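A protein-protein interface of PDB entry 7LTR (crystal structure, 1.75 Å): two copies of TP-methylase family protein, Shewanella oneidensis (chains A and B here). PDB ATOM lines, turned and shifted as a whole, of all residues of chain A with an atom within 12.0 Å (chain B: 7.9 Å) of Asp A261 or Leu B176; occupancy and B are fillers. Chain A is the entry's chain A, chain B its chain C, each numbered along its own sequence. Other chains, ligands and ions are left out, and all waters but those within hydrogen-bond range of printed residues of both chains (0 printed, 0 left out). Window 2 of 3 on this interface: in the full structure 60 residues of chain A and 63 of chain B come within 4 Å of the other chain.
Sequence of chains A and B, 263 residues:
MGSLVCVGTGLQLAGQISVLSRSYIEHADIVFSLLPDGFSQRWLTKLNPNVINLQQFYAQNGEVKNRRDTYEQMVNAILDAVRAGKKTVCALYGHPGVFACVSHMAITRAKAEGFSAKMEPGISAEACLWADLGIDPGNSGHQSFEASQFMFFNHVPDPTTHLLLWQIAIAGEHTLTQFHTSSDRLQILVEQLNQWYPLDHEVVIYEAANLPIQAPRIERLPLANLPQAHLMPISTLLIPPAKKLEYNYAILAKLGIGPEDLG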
ATOM      1  N   TYR A 247       3.281  16.391 -22.961  1.00  0.00           N
ATOM      2  CA  TYR A 247       2.280  17.437 -22.635  1.00  0.00           C
ATOM      3  C   TYR A 247       0.955  16.770 -22.272  1.00  0.00           C
ATOM      4  O   TYR A 247       0.533  15.809 -22.950  1.00  0.00           O
ATOM      5  CB  TYR A 247       2.092  18.411 -23.797  1.00  0.00           C
ATOM      6  CG  TYR A 247       3.357  19.126 -24.187  1.00  0.00           C
ATOM      7  CD1 TYR A 247       3.978  20.001 -23.312  1.00  0.00           C
ATOM      8  CD2 TYR A 247       3.947  18.908 -25.419  1.00  0.00           C
ATOM      9  CE1 TYR A 247       5.149  20.652 -23.656  1.00  0.00           C
ATOM     10  CE2 TYR A 247       5.118  19.552 -25.779  1.00  0.00           C
ATOM     11  CZ  TYR A 247       5.721  20.427 -24.895  1.00  0.00           C
ATOM     12  OH  TYR A 247       6.876  21.066 -25.244  1.00  0.00           O
ATOM     13  N   ASN A 248       0.325  17.291 -21.223  1.00  0.00           N
ATOM     14  CA  ASN A 248      -1.048  16.934 -20.790  1.00  0.00           C
ATOM     15  C   ASN A 248      -2.035  17.773 -21.613  1.00  0.00           C
ATOM     16  O   ASN A 248      -2.617  18.718 -21.054  1.00  0.00           O
ATOM     17  CB  ASN A 248      -1.189  17.153 -19.283  1.00  0.00           C
ATOM     18  CG  ASN A 248      -2.298  16.334 -18.664  1.00  0.00           C
ATOM     19  OD1 ASN A 248      -3.272  15.993 -19.332  1.00  0.00           O
ATOM     20  ND2 ASN A 248      -2.158  16.021 -17.386  1.00  0.00           N
ATOM     21  N   TYR A 249      -2.195  17.454 -22.902  1.00  0.00           N
ATOM     22  CA  TYR A 249      -2.959  18.273 -23.883  1.00  0.00           C
ATOM     23  C   TYR A 249      -4.383  18.521 -23.369  1.00  0.00           C
ATOM     24  O   TYR A 249      -4.897  19.640 -23.562  1.00  0.00           O
ATOM     25  CB  TYR A 249      -2.958  17.611 -25.263  1.00  0.00           C
ATOM     26  CG  TYR A 249      -1.625  17.656 -25.966  1.00  0.00           C
ATOM     27  CD1 TYR A 249      -1.127  18.843 -26.479  1.00  0.00           C
ATOM     28  CD2 TYR A 249      -0.859  16.515 -26.115  1.00  0.00           C
ATOM     29  CE1 TYR A 249       0.100  18.893 -27.120  1.00  0.00           C
ATOM     30  CE2 TYR A 249       0.369  16.547 -26.754  1.00  0.00           C
ATOM     31  CZ  TYR A 249       0.849  17.741 -27.262  1.00  0.00           C
ATOM     32  OH  TYR A 249       2.058  17.782 -27.893  1.00  0.00           O
ATOM     33  N   ILE A 251      -5.516  18.863 -20.278  1.00  0.00           N
ATOM     34  CA  ILE A 251      -5.533  19.848 -19.153  1.00  0.00           C
ATOM     35  C   ILE A 251      -5.050  21.213 -19.658  1.00  0.00           C
ATOM     36  O   ILE A 251      -5.647  22.230 -19.258  1.00  0.00           O
ATOM     37  CB  ILE A 251      -4.691  19.347 -17.963  1.00  0.00           C
ATOM     38  CG1 ILE A 251      -5.137  17.958 -17.498  1.00  0.00           C
ATOM     39  CG2 ILE A 251      -4.716  20.359 -16.826  1.00  0.00           C
ATOM     40  CD1 ILE A 251      -6.618  17.849 -17.218  1.00  0.00           C
ATOM     41  N   LEU A 252      -4.009  21.235 -20.497  1.00  0.00           N
ATOM     42  CA  LEU A 252      -3.471  22.479 -21.111  1.00  0.00           C
ATOM     43  C   LEU A 252      -4.597  23.188 -21.869  1.00  0.00           C
ATOM     44  O   LEU A 252      -4.657  24.431 -21.807  1.00  0.00           O
ATOM     45  CB  LEU A 252      -2.313  22.126 -22.049  1.00  0.00           C
ATOM     46  CG  LEU A 252      -1.042  21.640 -21.358  1.00  0.00           C
ATOM     47  CD1 LEU A 252      -0.028  21.145 -22.377  1.00  0.00           C
ATOM     48  CD2 LEU A 252      -0.444  22.736 -20.490  1.00  0.00           C
ATOM     49  N   ALA A 253      -5.452  22.415 -22.545  1.00  0.00           N
ATOM     50  CA  ALA A 253      -6.618  22.900 -23.322  1.00  0.00           C
ATOM     51  C   ALA A 253      -7.615  23.581 -22.376  1.00  0.00           C
ATOM     52  O   ALA A 253      -8.089  24.681 -22.718  1.00  0.00           O
ATOM     53  CB  ALA A 253      -7.251  21.754 -24.071  1.00  0.00           C
ATOM     54  N   LYS A 254      -7.914  22.955 -21.232  1.00  0.00           N
ATOM     55  CA  LYS A 254      -8.855  23.496 -20.213  1.00  0.00           C
ATOM     56  C   LYS A 254      -8.288  24.797 -19.634  1.00  0.00           C
ATOM     57  O   LYS A 254      -9.086  25.714 -19.364  1.00  0.00           O
ATOM     58  CB  LYS A 254      -9.105  22.489 -19.085  1.00  0.00           C
ATOM     59  CG  LYS A 254      -9.722  21.167 -19.516  1.00  0.00           C
ATOM     60  CD  LYS A 254     -10.498  20.482 -18.413  1.00  0.00           C
ATOM     61  CE  LYS A 254     -11.122  19.176 -18.857  1.00  0.00           C
ATOM     62  NZ  LYS A 254     -11.573  18.366 -17.700  1.00  0.00           N
ATOM     63  N   LEU A 255      -6.966  24.864 -19.440  1.00  0.00           N
ATOM     64  CA  LEU A 255      -6.266  26.049 -18.869  1.00  0.00           C
ATOM     65  C   LEU A 255      -6.179  27.152 -19.929  1.00  0.00           C
ATOM     66  O   LEU A 255      -5.930  28.312 -19.552  1.00  0.00           O
ATOM     67  CB  LEU A 255      -4.863  25.648 -18.404  1.00  0.00           C
ATOM     68  CG  LEU A 255      -4.787  24.841 -17.109  1.00  0.00           C
ATOM     69  CD1 LEU A 255      -3.341  24.508 -16.780  1.00  0.00           C
ATOM     70  CD2 LEU A 255      -5.436  25.590 -15.955  1.00  0.00           C
ATOM     71  N   GLY A 256      -6.359  26.789 -21.202  1.00  0.00           N
ATOM     72  CA  GLY A 256      -6.269  27.711 -22.350  1.00  0.00           C
ATOM     73  C   GLY A 256      -4.828  28.041 -22.703  1.00  0.00           C
ATOM     74  O   GLY A 256      -4.618  29.039 -23.417  1.00  0.00           O
ATOM     75  N   ILE A 257      -3.868  27.240 -22.228  1.00  0.00           N
ATOM     76  CA  ILE A 257      -2.413  27.430 -22.519  1.00  0.00           C
ATOM     77  C   ILE A 257      -1.983  26.377 -23.547  1.00  0.00           C
ATOM     78  O   ILE A 257      -2.596  25.293 -23.578  1.00  0.00           O
ATOM     79  CB  ILE A 257      -1.559  27.380 -21.233  1.00  0.00           C
ATOM     80  CG1 ILE A 257      -0.527  26.251 -21.253  1.00  0.00           C
ATOM     81  CG2 ILE A 257      -2.439  27.316 -19.995  1.00  0.00           C
ATOM     82  CD1 ILE A 257       0.670  26.511 -20.364  1.00  0.00           C
ATOM     83  N   GLY A 258      -0.979  26.705 -24.364  1.00  0.00           N
ATOM     84  CA  GLY A 258      -0.451  25.828 -25.426  1.00  0.00           C
ATOM     85  C   GLY A 258       0.921  25.271 -25.060  1.00  0.00           C
ATOM     86  O   GLY A 258       1.622  25.835 -24.223  1.00  0.00           O
ATOM     87  N   PRO A 259       1.339  24.141 -25.671  1.00  0.00           N
ATOM     88  CA  PRO A 259       2.671  23.587 -25.434  1.00  0.00           C
ATOM     89  C   PRO A 259       3.758  24.645 -25.674  1.00  0.00           C
ATOM     90  O   PRO A 259       4.592  24.844 -24.810  1.00  0.00           O
ATOM     91  CB  PRO A 259       2.796  22.451 -26.460  1.00  0.00           C
ATOM     92  CG  PRO A 259       1.365  22.076 -26.797  1.00  0.00           C
ATOM     93  CD  PRO A 259       0.555  23.345 -26.627  1.00  0.00           C
ATOM     94  N   GLU A 260       3.706  25.288 -26.845  1.00  0.00           N
ATOM     95  CA  GLU A 260       4.638  26.362 -27.280  1.00  0.00           C
ATOM     96  C   GLU A 260       4.984  27.270 -26.093  1.00  0.00           C
ATOM     97  O   GLU A 260       6.132  27.751 -26.037  1.00  0.00           O
ATOM     98  CB  GLU A 260       4.002  27.179 -28.408  1.00  0.00           C
ATOM     99  CG  GLU A 260       2.512  27.403 -28.228  1.00  0.00           C
ATOM    100  CD  GLU A 260       1.634  26.556 -29.133  1.00  0.00           C
ATOM    101  OE1 GLU A 260       0.660  25.965 -28.626  1.00  0.00           O
ATOM    102  OE2 GLU A 260       1.924  26.496 -30.346  1.00  0.00           O
ATOM    103  N   ASP A 261       4.026  27.488 -25.186  1.00  0.00           N
ATOM    104  CA  ASP A 261       4.129  28.459 -24.061  1.00  0.00           C
ATOM    105  C   ASP A 261       5.019  27.907 -22.940  1.00  0.00           C
ATOM    106  O   ASP A 261       5.503  28.725 -22.132  1.00  0.00           O
ATOM    107  CB  ASP A 261       2.752  28.812 -23.494  1.00  0.00           C
ATOM    108  CG  ASP A 261       1.727  29.191 -24.549  1.00  0.00           C
ATOM    109  OD1 ASP A 261       2.036  30.071 -25.377  1.00  0.00           O
ATOM    110  OD2 ASP A 261       0.629  28.599 -24.535  1.00  0.00           O
ATOM    111  N   LEU A 262       5.219  26.586 -22.870  1.00  0.00           N
ATOM    112  CA  LEU A 262       6.054  25.953 -21.812  1.00  0.00           C
ATOM    113  C   LEU A 262       7.463  25.705 -22.364  1.00  0.00           C
ATOM    114  O   LEU A 262       8.236  26.641 -22.565  1.00  0.00           O
ATOM    115  CB  LEU A 262       5.408  24.643 -21.345  1.00  0.00           C
ATOM    116  CG  LEU A 262       3.901  24.690 -21.095  1.00  0.00           C
ATOM    117  CD1 LEU A 262       3.326  23.284 -21.032  1.00  0.00           C
ATOM    118  CD2 LEU A 262       3.577  25.451 -19.820  1.00  0.00           C
ATOM    119  N   PHE B 152       0.498  20.186 -16.303  1.00  0.00           N
ATOM    120  CA  PHE B 152       1.070  20.506 -17.639  1.00  0.00           C
ATOM    121  C   PHE B 152       1.524  19.229 -18.350  1.00  0.00           C
ATOM    122  O   PHE B 152       1.460  19.191 -19.594  1.00  0.00           O
ATOM    123  CB  PHE B 152       2.268  21.455 -17.533  1.00  0.00           C
ATOM    124  CG  PHE B 152       1.959  22.830 -17.000  1.00  0.00           C
ATOM    125  CD1 PHE B 152       0.657  23.303 -16.947  1.00  0.00           C
ATOM    126  CD2 PHE B 152       2.981  23.663 -16.573  1.00  0.00           C
ATOM    127  CE1 PHE B 152       0.384  24.572 -16.460  1.00  0.00           C
ATOM    128  CE2 PHE B 152       2.706  24.931 -16.088  1.00  0.00           C
ATOM    129  CZ  PHE B 152       1.408  25.382 -16.032  1.00  0.00           C
ATOM    130  N   GLY B 172      -1.195  25.496 -12.090  1.00  0.00           N
ATOM    131  CA  GLY B 172      -1.630  25.843 -13.456  1.00  0.00           C
ATOM    132  C   GLY B 172      -1.409  27.313 -13.767  1.00  0.00           C
ATOM    133  O   GLY B 172      -1.751  27.730 -14.893  1.00  0.00           O
ATOM    134  N   GLU B 173      -0.862  28.071 -12.811  1.00  0.00           N
ATOM    135  CA  GLU B 173      -0.537  29.514 -12.972  1.00  0.00           C
ATOM    136  C   GLU B 173       0.532  29.657 -14.061  1.00  0.00           C
ATOM    137  O   GLU B 173       1.494  28.864 -14.057  1.00  0.00           O
ATOM    138  CB  GLU B 173      -0.073  30.125 -11.649  1.00  0.00           C
ATOM    139  CG  GLU B 173       0.095  31.634 -11.711  1.00  0.00           C
ATOM    140  CD  GLU B 173      -0.467  32.386 -10.514  1.00  0.00           C
ATOM    141  OE1 GLU B 173      -1.025  31.729  -9.613  1.00  0.00           O
ATOM    142  OE2 GLU B 173      -0.349  33.627 -10.491  1.00  0.00           O
ATOM    143  N   HIS B 174       0.357  30.631 -14.957  1.00  0.00           N
ATOM    144  CA  HIS B 174       1.220  30.863 -16.146  1.00  0.00           C
ATOM    145  C   HIS B 174       0.886  32.234 -16.747  1.00  0.00           C
ATOM    146  O   HIS B 174      -0.263  32.686 -16.563  1.00  0.00           O
ATOM    147  CB  HIS B 174       1.027  29.715 -17.148  1.00  0.00           C
ATOM    148  CG  HIS B 174       1.958  29.750 -18.313  1.00  0.00           C
ATOM    149  ND1 HIS B 174       1.644  30.403 -19.489  1.00  0.00           N
ATOM    150  CD2 HIS B 174       3.178  29.201 -18.498  1.00  0.00           C
ATOM    151  CE1 HIS B 174       2.635  30.263 -20.344  1.00  0.00           C
ATOM    152  NE2 HIS B 174       3.590  29.529 -19.760  1.00  0.00           N
ATOM    153  N   THR B 175       1.845  32.871 -17.428  1.00  0.00           N
ATOM    154  CA  THR B 175       1.656  34.187 -18.097  1.00  0.00           C
ATOM    155  C   THR B 175       0.358  34.150 -18.911  1.00  0.00           C
ATOM    156  O   THR B 175      -0.388  35.149 -18.875  1.00  0.00           O
ATOM    157  CB  THR B 175       2.849  34.562 -18.986  1.00  0.00           C
ATOM    158  OG1 THR B 175       3.525  33.361 -19.363  1.00  0.00           O
ATOM    159  CG2 THR B 175       3.817  35.502 -18.302  1.00  0.00           C
ATOM    160  N   LEU B 176       0.104  33.037 -19.608  1.00  0.00           N
ATOM    161  CA  LEU B 176      -1.105  32.828 -20.449  1.00  0.00           C
ATOM    162  C   LEU B 176      -2.350  32.728 -19.557  1.00  0.00           C
ATOM    163  O   LEU B 176      -3.393  33.287 -19.948  1.00  0.00           O
ATOM    164  CB  LEU B 176      -0.924  31.563 -21.296  1.00  0.00           C
ATOM    165  CG  LEU B 176      -0.598  31.800 -22.770  1.00  0.00           C
ATOM    166  CD1 LEU B 176      -1.764  32.467 -23.486  1.00  0.00           C
ATOM    167  CD2 LEU B 176       0.668  32.629 -22.927  1.00  0.00           C
ATOM    168  N   THR B 177      -2.247  32.049 -18.409  1.00  0.00           N
ATOM    169  CA  THR B 177      -3.381  31.793 -17.478  1.00  0.00           C
ATOM    170  C   THR B 177      -3.327  32.732 -16.267  1.00  0.00           C
ATOM    171  O   THR B 177      -3.856  32.334 -15.211  1.00  0.00           O
ATOM    172  CB  THR B 177      -3.384  30.353 -16.949  1.00  0.00           C
ATOM    173  OG1 THR B 177      -2.328  30.231 -15.996  1.00  0.00           O
ATOM    174  CG2 THR B 177      -3.217  29.316 -18.038  1.00  0.00           C
ATOM    175  N   GLN B 178      -2.726  33.920 -16.395  1.00  0.00           N
ATOM    176  CA  GLN B 178      -2.553  34.847 -15.243  1.00  0.00           C
ATOM    177  C   GLN B 178      -3.897  35.494 -14.889  1.00  0.00           C
ATOM    178  O   GLN B 178      -4.065  35.884 -13.716  1.00  0.00           O
ATOM    179  CB  GLN B 178      -1.501  35.926 -15.508  1.00  0.00           C
ATOM    180  CG  GLN B 178      -1.190  36.736 -14.259  1.00  0.00           C
ATOM    181  CD  GLN B 178      -1.000  35.841 -13.060  1.00  0.00           C
ATOM    182  OE1 GLN B 178      -1.145  36.263 -11.914  1.00  0.00           O
ATOM    183  NE2 GLN B 178      -0.681  34.583 -13.319  1.00  0.00           N
ATOM    184  N   PHE B 179      -4.809  35.612 -15.858  1.00  0.00           N
ATOM    185  CA  PHE B 179      -6.190  36.124 -15.652  1.00  0.00           C
ATOM    186  C   PHE B 179      -7.181  34.963 -15.791  1.00  0.00           C
ATOM    187  O   PHE B 179      -7.915  34.916 -16.798  1.00  0.00           O
ATOM    188  CB  PHE B 179      -6.508  37.268 -16.621  1.00  0.00           C
ATOM    189  CG  PHE B 179      -5.740  37.251 -17.920  1.00  0.00           C
ATOM    190  CD1 PHE B 179      -5.616  36.087 -18.661  1.00  0.00           C
ATOM    191  CD2 PHE B 179      -5.160  38.409 -18.413  1.00  0.00           C
ATOM    192  CE1 PHE B 179      -4.913  36.079 -19.857  1.00  0.00           C
ATOM    193  CE2 PHE B 179      -4.461  38.401 -19.610  1.00  0.00           C
ATOM    194  CZ  PHE B 179      -4.339  37.236 -20.330  1.00  0.00           C
ATOM    195  N   HIS B 180      -7.200  34.060 -14.803  1.00  0.00           N
ATOM    196  CA  HIS B 180      -7.980  32.791 -14.822  1.00  0.00           C
ATOM    197  C   HIS B 180      -8.644  32.547 -13.457  1.00  0.00           C
ATOM    198  O   HIS B 180      -9.675  31.847 -13.418  1.00  0.00           O
ATOM    199  CB  HIS B 180      -7.066  31.627 -15.229  1.00  0.00           C
ATOM    200  CG  HIS B 180      -7.709  30.663 -16.169  1.00  0.00           C
ATOM    201  ND1 HIS B 180      -8.980  30.167 -15.959  1.00  0.00           N
ATOM    202  CD2 HIS B 180      -7.265  30.101 -17.314  1.00  0.00           C
ATOM    203  CE1 HIS B 180      -9.294  29.343 -16.939  1.00  0.00           C
ATOM    204  NE2 HIS B 180      -8.258  29.285 -17.782  1.00  0.00           N
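Of the printed residues of chain A, Leu B176 touches Asp A261 (3.8 Å).
No residue of chain B comes within 4 Å of Gly A258.
Of the printed residues of chain A, His B174 touches Asp A261 (3.2 Å) and Leu A262 (3.996 Å).
Of the printed residues of chain A, Phe B152 touches Tyr A247 (3.6 Å), Asn A248 (2.7 Å), Leu A252 (3.7 Å), Leu A255 (3.7 Å) and Leu A262 (3.8 Å).
Of the printed residues of chain B, Ile A257 touches Thr B177.
The nearest residue of chain B that does not touch Asp A261 is Thr B175 (5.8 Å).
The nearest residue of chain A that does not touch Leu B176 is Ile A257 (4.2 Å).
The nearest printed residue of chain A that does not touch His B180 is Gly A256 (4.6 Å).
O of Gly B172 is in hydrogen-bond range of OG1 of Thr B177 (2.8 Å).
ND1 of His B174 sits at hydrogen-bond distance from N of Leu B176, at 3.1 Å.
The backbone NH (N) of Ile A257 lies within hydrogen-bond range of the backbone carbonyl oxygen (O) of Leu A252.
The backbone NH of Gly A258 lies within hydrogen-bond range of the side-chain carboxylate of Asp A261 (2.5 Å).
The backbone NH (N) of His B174 lies within hydrogen-bond range of the side-chain hydroxyl (OG1) of Thr B177, 2.9 Å away.
No position is printed for both chains.
Of the 13 pairs that touch across the chains among the printed residues, none has its exchanged pair printed and touching as well.
O of Leu A255 is in hydrogen-bond range of NE2 of His B180 (3.1 Å).
A ring nitrogen (NE2) of His B174 sits at hydrogen-bond distance from the backbone carbonyl oxygen (O) of Asp A261 (3.2 Å).
The backbone NH (N) of Asn A248 is in hydrogen-bond range of the backbone carbonyl oxygen (O) of Phe B152 (2.7 Å).
Of the 15 printed residues of chain A, 8 touch a printed residue of chain B.
Printed residues of chain A that touch a printed residue of chain B: Tyr A247, Asn A248, Leu A252, Lys A254, Leu A255, Ile A257, Asp A261 and Leu A262.
Hydrophobic or aromatic side chains of chain B within 4 Å of the printed part of chain A: Phe B152, His B174, Leu B176 and His B180.
Among the printed residues, 13 pairs touch across the chains.
Among the printed residues, no Asp or Glu carboxylate lies within 4 Å of a Lys or Arg side-chain nitrogen of the other chain.
Phe B152 touches Tyr A247 (O to CA, 3.6 Å).
Leu A252 touches Phe B152 (CD1 to O, 3.7 Å).
O of Lys A254 touches NE2 of His B180, 3.99 Å away.
Phe B152 touches Leu A255.
CD1 of Leu A255 touches CA of Gly B172, 3.97 Å away.
Leu A255 touches Thr B177.
Thr B177 touches Ile A257.
Asp A261 touches Leu B176.
Phe B152 touches Leu A262.
Leu A262 touches His B174.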
